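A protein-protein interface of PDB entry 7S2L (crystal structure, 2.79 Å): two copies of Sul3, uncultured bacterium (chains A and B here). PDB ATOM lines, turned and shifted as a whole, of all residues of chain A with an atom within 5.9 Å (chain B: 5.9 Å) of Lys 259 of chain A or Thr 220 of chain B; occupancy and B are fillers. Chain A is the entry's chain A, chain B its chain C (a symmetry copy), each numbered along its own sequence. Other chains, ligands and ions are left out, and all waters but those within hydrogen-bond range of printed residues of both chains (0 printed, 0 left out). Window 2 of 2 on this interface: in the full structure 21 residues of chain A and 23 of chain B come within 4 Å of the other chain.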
ATOM      1  N   MET A   3      10.781   1.490  13.179  1.00  0.00           N
ATOM      2  CA  MET A   3      10.050   2.334  14.116  1.00  0.00           C
ATOM      3  C   MET A   3       8.878   2.985  13.391  1.00  0.00           C
ATOM      4  O   MET A   3       9.062   3.568  12.317  1.00  0.00           O
ATOM      5  CB  MET A   3      10.971   3.404  14.722  1.00  0.00           C
ATOM      6  CG  MET A   3      10.238   4.540  15.429  1.00  0.00           C
ATOM      7  SD  MET A   3       9.807   4.125  17.145  1.00  0.00           S
ATOM      8  CE  MET A   3      10.773   5.364  18.057  1.00  0.00           C
ATOM      9  N   ASP A  39       7.269  17.853  19.548  1.00  0.00           N
ATOM     10  CA  ASP A  39       7.042  16.638  20.321  1.00  0.00           C
ATOM     11  C   ASP A  39       7.486  15.385  19.582  1.00  0.00           C
ATOM     12  O   ASP A  39       7.498  14.301  20.180  1.00  0.00           O
ATOM     13  CB  ASP A  39       5.564  16.512  20.696  1.00  0.00           C
ATOM     14  CG  ASP A  39       5.033  17.733  21.437  1.00  0.00           C
ATOM     15  OD1 ASP A  39       5.810  18.366  22.190  1.00  0.00           O
ATOM     16  OD2 ASP A  39       3.827  18.045  21.283  1.00  0.00           O
ATOM     17  N   LEU A 254       2.835   9.591  22.718  1.00  0.00           N
ATOM     18  CA  LEU A 254       3.198   8.458  21.880  1.00  0.00           C
ATOM     19  C   LEU A 254       4.705   8.382  21.698  1.00  0.00           C
ATOM     20  O   LEU A 254       5.296   7.298  21.793  1.00  0.00           O
ATOM     21  CB  LEU A 254       2.492   8.546  20.530  1.00  0.00           C
ATOM     22  CG  LEU A 254       2.845   7.415  19.557  1.00  0.00           C
ATOM     23  CD1 LEU A 254       2.610   6.050  20.205  1.00  0.00           C
ATOM     24  CD2 LEU A 254       2.091   7.548  18.229  1.00  0.00           C
ATOM     25  N   SER A 255       5.347   9.524  21.452  1.00  0.00           N
ATOM     26  CA  SER A 255       6.801   9.528  21.349  1.00  0.00           C
ATOM     27  C   SER A 255       7.433   8.957  22.611  1.00  0.00           C
ATOM     28  O   SER A 255       8.386   8.172  22.535  1.00  0.00           O
ATOM     29  CB  SER A 255       7.311  10.944  21.082  1.00  0.00           C
ATOM     30  OG  SER A 255       8.668  10.913  20.673  1.00  0.00           O
ATOM     31  N   ASP A 256       6.899   9.318  23.782  1.00  0.00           N
ATOM     32  CA  ASP A 256       7.438   8.778  25.026  1.00  0.00           C
ATOM     33  C   ASP A 256       7.233   7.276  25.093  1.00  0.00           C
ATOM     34  O   ASP A 256       8.141   6.535  25.489  1.00  0.00           O
ATOM     35  CB  ASP A 256       6.795   9.464  26.232  1.00  0.00           C
ATOM     36  CG  ASP A 256       7.063  10.958  26.256  1.00  0.00           C
ATOM     37  OD1 ASP A 256       7.612  11.469  25.254  1.00  0.00           O
ATOM     38  OD2 ASP A 256       6.776  11.619  27.278  1.00  0.00           O
ATOM     39  N   ALA A 257       6.049   6.804  24.692  1.00  0.00           N
ATOM     40  CA  ALA A 257       5.795   5.369  24.718  1.00  0.00           C
ATOM     41  C   ALA A 257       6.777   4.625  23.822  1.00  0.00           C
ATOM     42  O   ALA A 257       7.340   3.599  24.225  1.00  0.00           O
ATOM     43  CB  ALA A 257       4.351   5.085  24.308  1.00  0.00           C
ATOM     44  N   LEU A 258       7.029   5.154  22.620  1.00  0.00           N
ATOM     45  CA  LEU A 258       7.937   4.486  21.692  1.00  0.00           C
ATOM     46  C   LEU A 258       9.383   4.588  22.159  1.00  0.00           C
ATOM     47  O   LEU A 258      10.141   3.611  22.074  1.00  0.00           O
ATOM     48  CB  LEU A 258       7.788   5.080  20.294  1.00  0.00           C
ATOM     49  CG  LEU A 258       6.797   4.438  19.320  1.00  0.00           C
ATOM     50  CD1 LEU A 258       5.513   3.962  19.998  1.00  0.00           C
ATOM     51  CD2 LEU A 258       6.488   5.426  18.212  1.00  0.00           C
ATOM     52  N   LYS A 259       9.783   5.764  22.649  1.00  0.00           N
ATOM     53  CA  LYS A 259      11.131   5.928  23.182  1.00  0.00           C
ATOM     54  C   LYS A 259      11.402   4.947  24.320  1.00  0.00           C
ATOM     55  O   LYS A 259      12.460   4.304  24.352  1.00  0.00           O
ATOM     56  CB  LYS A 259      11.328   7.369  23.648  1.00  0.00           C
ATOM     57  CG  LYS A 259      11.747   8.324  22.550  1.00  0.00           C
ATOM     58  CD  LYS A 259      11.416   9.764  22.915  1.00  0.00           C
ATOM     59  CE  LYS A 259      12.521  10.701  22.465  1.00  0.00           C
ATOM     60  NZ  LYS A 259      12.005  11.860  21.689  1.00  0.00           N
ATOM     61  N   ILE A 260      10.457   4.808  25.255  1.00  0.00           N
ATOM     62  CA  ILE A 260      10.649   3.878  26.368  1.00  0.00           C
ATOM     63  C   ILE A 260      10.704   2.447  25.861  1.00  0.00           C
ATOM     64  O   ILE A 260      11.517   1.640  26.331  1.00  0.00           O
ATOM     65  CB  ILE A 260       9.545   4.048  27.431  1.00  0.00           C
ATOM     66  CG1 ILE A 260       9.696   5.376  28.170  1.00  0.00           C
ATOM     67  CG2 ILE A 260       9.540   2.880  28.409  1.00  0.00           C
ATOM     68  CD1 ILE A 260      10.928   5.444  29.034  1.00  0.00           C
ATOM     69  N   SER A 261       9.852   2.112  24.884  1.00  0.00           N
ATOM     70  CA  SER A 261       9.750   0.729  24.422  1.00  0.00           C
ATOM     71  C   SER A 261      10.971   0.318  23.611  1.00  0.00           C
ATOM     72  O   SER A 261      11.449  -0.818  23.728  1.00  0.00           O
ATOM     73  CB  SER A 261       8.477   0.545  23.597  1.00  0.00           C
ATOM     74  OG  SER A 261       7.421   1.330  24.119  1.00  0.00           O
ATOM     75  N   LYS A 262      11.488   1.224  22.778  1.00  0.00           N
ATOM     76  CA  LYS A 262      12.696   0.906  22.028  1.00  0.00           C
ATOM     77  C   LYS A 262      13.898   0.763  22.954  1.00  0.00           C
ATOM     78  O   LYS A 262      14.751  -0.104  22.735  1.00  0.00           O
ATOM     79  CB  LYS A 262      12.953   1.970  20.963  1.00  0.00           C
ATOM     80  CG  LYS A 262      14.073   1.618  19.992  1.00  0.00           C
ATOM     81  CD  LYS A 262      14.838   2.865  19.574  1.00  0.00           C
ATOM     82  CE  LYS A 262      15.796   2.585  18.425  1.00  0.00           C
ATOM     83  NZ  LYS A 262      16.559   3.813  18.040  1.00  0.00           N
ATOM     84  N   ALA A 263      13.977   1.591  24.003  1.00  0.00           N
ATOM     85  CA  ALA A 263      15.097   1.496  24.940  1.00  0.00           C
ATOM     86  C   ALA A 263      15.080   0.175  25.700  1.00  0.00           C
ATOM     87  O   ALA A 263      16.137  -0.424  25.940  1.00  0.00           O
ATOM     88  CB  ALA A 263      15.074   2.670  25.917  1.00  0.00           C
ATOM     89  N   LEU A 264      13.893  -0.290  26.096  1.00  0.00           N
ATOM     90  CA  LEU A 264      13.784  -1.585  26.757  1.00  0.00           C
ATOM     91  C   LEU A 264      13.899  -2.725  25.752  1.00  0.00           C
ATOM     92  O   LEU A 264      14.607  -3.710  25.995  1.00  0.00           O
ATOM     93  CB  LEU A 264      12.464  -1.673  27.522  1.00  0.00           C
ATOM     94  CG  LEU A 264      12.196  -0.505  28.468  1.00  0.00           C
ATOM     95  CD1 LEU A 264      10.757  -0.493  28.916  1.00  0.00           C
ATOM     96  CD2 LEU A 264      13.146  -0.575  29.660  1.00  0.00           C
ATOM     97  N   PHE B 215      14.579   8.090  36.118  1.00  0.00           N
ATOM     98  CA  PHE B 215      15.374   7.521  35.035  1.00  0.00           C
ATOM     99  C   PHE B 215      14.572   7.433  33.745  1.00  0.00           C
ATOM    100  O   PHE B 215      15.148   7.511  32.653  1.00  0.00           O
ATOM    101  CB  PHE B 215      15.908   6.148  35.437  1.00  0.00           C
ATOM    102  CG  PHE B 215      14.920   5.035  35.257  1.00  0.00           C
ATOM    103  CD1 PHE B 215      13.994   4.747  36.250  1.00  0.00           C
ATOM    104  CD2 PHE B 215      14.913   4.278  34.096  1.00  0.00           C
ATOM    105  CE1 PHE B 215      13.086   3.722  36.088  1.00  0.00           C
ATOM    106  CE2 PHE B 215      14.011   3.263  33.925  1.00  0.00           C
ATOM    107  CZ  PHE B 215      13.098   2.980  34.920  1.00  0.00           C
ATOM    108  N   LEU B 216      13.248   7.275  33.846  1.00  0.00           N
ATOM    109  CA  LEU B 216      12.412   7.337  32.651  1.00  0.00           C
ATOM    110  C   LEU B 216      12.585   8.668  31.923  1.00  0.00           C
ATOM    111  O   LEU B 216      12.519   8.717  30.688  1.00  0.00           O
ATOM    112  CB  LEU B 216      10.943   7.103  33.022  1.00  0.00           C
ATOM    113  CG  LEU B 216      10.612   5.785  33.746  1.00  0.00           C
ATOM    114  CD1 LEU B 216       9.228   5.828  34.376  1.00  0.00           C
ATOM    115  CD2 LEU B 216      10.729   4.592  32.812  1.00  0.00           C
ATOM    116  N   GLY B 217      12.836   9.749  32.664  1.00  0.00           N
ATOM    117  CA  GLY B 217      13.091  11.031  32.033  1.00  0.00           C
ATOM    118  C   GLY B 217      14.380  11.068  31.238  1.00  0.00           C
ATOM    119  O   GLY B 217      14.491  11.828  30.273  1.00  0.00           O
ATOM    120  N   LYS B 218      15.374  10.267  31.633  1.00  0.00           N
ATOM    121  CA  LYS B 218      16.603  10.212  30.851  1.00  0.00           C
ATOM    122  C   LYS B 218      16.345   9.606  29.474  1.00  0.00           C
ATOM    123  O   LYS B 218      16.863  10.098  28.464  1.00  0.00           O
ATOM    124  CB  LYS B 218      17.682   9.423  31.605  1.00  0.00           C
ATOM    125  CG  LYS B 218      19.015   9.261  30.836  1.00  0.00           C
ATOM    126  CD  LYS B 218      19.047   7.984  29.966  1.00  0.00           C
ATOM    127  CE  LYS B 218      20.403   7.743  29.307  1.00  0.00           C
ATOM    128  NZ  LYS B 218      20.505   6.367  28.730  1.00  0.00           N
ATOM    129  N   ILE B 219      15.547   8.538  29.421  1.00  0.00           N
ATOM    130  CA  ILE B 219      15.229   7.886  28.154  1.00  0.00           C
ATOM    131  C   ILE B 219      14.404   8.812  27.272  1.00  0.00           C
ATOM    132  O   ILE B 219      14.588   8.864  26.048  1.00  0.00           O
ATOM    133  CB  ILE B 219      14.488   6.563  28.424  1.00  0.00           C
ATOM    134  CG1 ILE B 219      15.373   5.608  29.225  1.00  0.00           C
ATOM    135  CG2 ILE B 219      14.027   5.918  27.134  1.00  0.00           C
ATOM    136  CD1 ILE B 219      14.629   4.406  29.745  1.00  0.00           C
ATOM    137  N   THR B 220      13.495   9.566  27.879  1.00  0.00           N
ATOM    138  CA  THR B 220      12.462  10.281  27.146  1.00  0.00           C
ATOM    139  C   THR B 220      12.768  11.752  26.916  1.00  0.00           C
ATOM    140  O   THR B 220      12.547  12.258  25.812  1.00  0.00           O
ATOM    141  CB  THR B 220      11.139  10.171  27.890  1.00  0.00           C
ATOM    142  OG1 THR B 220      10.837   8.793  28.129  1.00  0.00           O
ATOM    143  CG2 THR B 220      10.083  10.754  27.055  1.00  0.00           C
ATOM    144  N   GLY B 221      13.252  12.459  27.930  1.00  0.00           N
ATOM    145  CA  GLY B 221      13.422  13.892  27.802  1.00  0.00           C
ATOM    146  C   GLY B 221      12.171  14.686  28.099  1.00  0.00           C
ATOM    147  O   GLY B 221      11.999  15.785  27.559  1.00  0.00           O
ATOM    148  N   THR B 222      11.285  14.162  28.941  1.00  0.00           N
ATOM    149  CA  THR B 222      10.074  14.869  29.320  1.00  0.00           C
ATOM    150  C   THR B 222       9.929  14.838  30.838  1.00  0.00           C
ATOM    151  O   THR B 222      10.772  14.297  31.557  1.00  0.00           O
ATOM    152  CB  THR B 222       8.837  14.258  28.653  1.00  0.00           C
ATOM    153  OG1 THR B 222       8.840  12.840  28.855  1.00  0.00           O
ATOM    154  CG2 THR B 222       8.853  14.544  27.165  1.00  0.00           C
ATOM    155  N   VAL B 224       8.557  13.303  33.642  1.00  0.00           N
ATOM    156  CA  VAL B 224       7.927  12.063  34.076  1.00  0.00           C
ATOM    157  C   VAL B 224       7.240  12.197  35.432  1.00  0.00           C
ATOM    158  O   VAL B 224       6.354  11.393  35.746  1.00  0.00           O
ATOM    159  CB  VAL B 224       8.965  10.927  34.119  1.00  0.00           C
ATOM    160  CG1 VAL B 224       9.676  10.813  32.780  1.00  0.00           C
ATOM    161  CG2 VAL B 224       9.956  11.155  35.251  1.00  0.00           C
ATOM    162  N   ARG B 227       3.665  13.311  34.419  1.00  0.00           N
ATOM    163  CA  ARG B 227       3.138  12.813  33.135  1.00  0.00           C
ATOM    164  C   ARG B 227       2.883  11.313  33.088  1.00  0.00           C
ATOM    165  O   ARG B 227       3.662  10.541  33.594  1.00  0.00           O
ATOM    166  CB  ARG B 227       4.023  13.254  31.984  1.00  0.00           C
ATOM    167  CG  ARG B 227       3.575  14.558  31.371  1.00  0.00           C
ATOM    168  CD  ARG B 227       4.468  14.989  30.238  1.00  0.00           C
ATOM    169  NE  ARG B 227       4.797  13.883  29.364  1.00  0.00           N
ATOM    170  CZ  ARG B 227       4.202  13.651  28.205  1.00  0.00           C
ATOM    171  NH1 ARG B 227       3.239  14.446  27.790  1.00  0.00           N
ATOM    172  NH2 ARG B 227       4.575  12.626  27.464  1.00  0.00           N
ATOM    173  N   PRO B 230       5.356   8.091  29.950  1.00  0.00           N
ATOM    174  CA  PRO B 230       6.618   7.352  30.102  1.00  0.00           C
ATOM    175  C   PRO B 230       6.564   6.353  31.235  1.00  0.00           C
ATOM    176  O   PRO B 230       7.172   5.279  31.140  1.00  0.00           O
ATOM    177  CB  PRO B 230       7.653   8.463  30.340  1.00  0.00           C
ATOM    178  CG  PRO B 230       6.876   9.593  30.884  1.00  0.00           C
ATOM    179  CD  PRO B 230       5.529   9.527  30.250  1.00  0.00           C
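Asp 256 of chain A touches Thr 220 of chain B. Asp 256 of chain A touches Pro 230 of chain B (OD2 to CD, 3.8 Å). Lys 259 of chain A touches Ile 219 of chain B (O to CG2, 3.6 Å). Thr 220 of chain B touches Lys 259 of chain A (O to CE, 3.7 Å). Ile 260 of chain A touches Leu 216 of chain B. CD1 of Ile 260 of chain A touches CG2 of Ile 219 of chain B, 3.7 Å away. Ile 260 of chain A touches Thr 220 of chain B (CD1 to OG1, 3.5 Å). Ile 260 of chain A touches Pro 230 of chain B (CG1 to O, 3.9 Å). Ala 263 of chain A touches Ile 219 of chain B.
Of the 13 printed residues of chain A, 4 touch a printed residue of chain B. Among the printed residues, 11 pairs touch across the chains. Among the printed residues, Asp or Glu carboxylates within 4 Å of a Lys or Arg side-chain nitrogen of the other chain: Asp 256 of chain A with Arg 227 of chain B (2.4 Å).
The side-chain hydroxyl (OG1) of Thr 222 of chain B lies within hydrogen-bond range of the side-chain carboxylate (OD2) of Asp 256 of chain A (2.9 Å). NH2 of Arg 227 of chain B lies within salt-bridge range of OD2 of Asp 256 of chain A, at 2.4 Å.
Ser 255 of chain A touches none of the printed residues of chain B. Lys 259 of chain A touches just these residues of chain B: Ile 219 and Thr 220. Of the printed residues of chain B, Ile 260 of chain A touches Leu 216, Ile 219, Thr 220 and Pro 230. Of the printed residues of chain A, Leu 216 of chain B touches Ile 260. Of the printed residues of chain A, Ile 219 of chain B touches Lys 259 (3.6 Å), Ile 260 (3.7 Å) and Ala 263 (3.6 Å). Of the printed residues of chain A, Thr 220 of chain B touches Asp 256 (3.1 Å), Lys 259 (3.7 Å) and Ile 260 (3.5 Å). Gly 221 of chain B touches none of the printed residues of chain A. Printed residues of chain A within 4 Å of Thr 222 of chain B: Asp 256 (2.9 Å). Printed residues of chain A within 4 Å of Pro 230 of chain B: Asp 256 and Ile 260.
The side-chain hydroxyl of Thr 220 of chain B sits at hydrogen-bond distance from the backbone carbonyl oxygen of Leu 216 of chain B (3.1 Å).
No position is printed for both chains. Of the 11 pairs that touch across the chains among the printed residues, none has its exchanged pair printed and touching as well.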
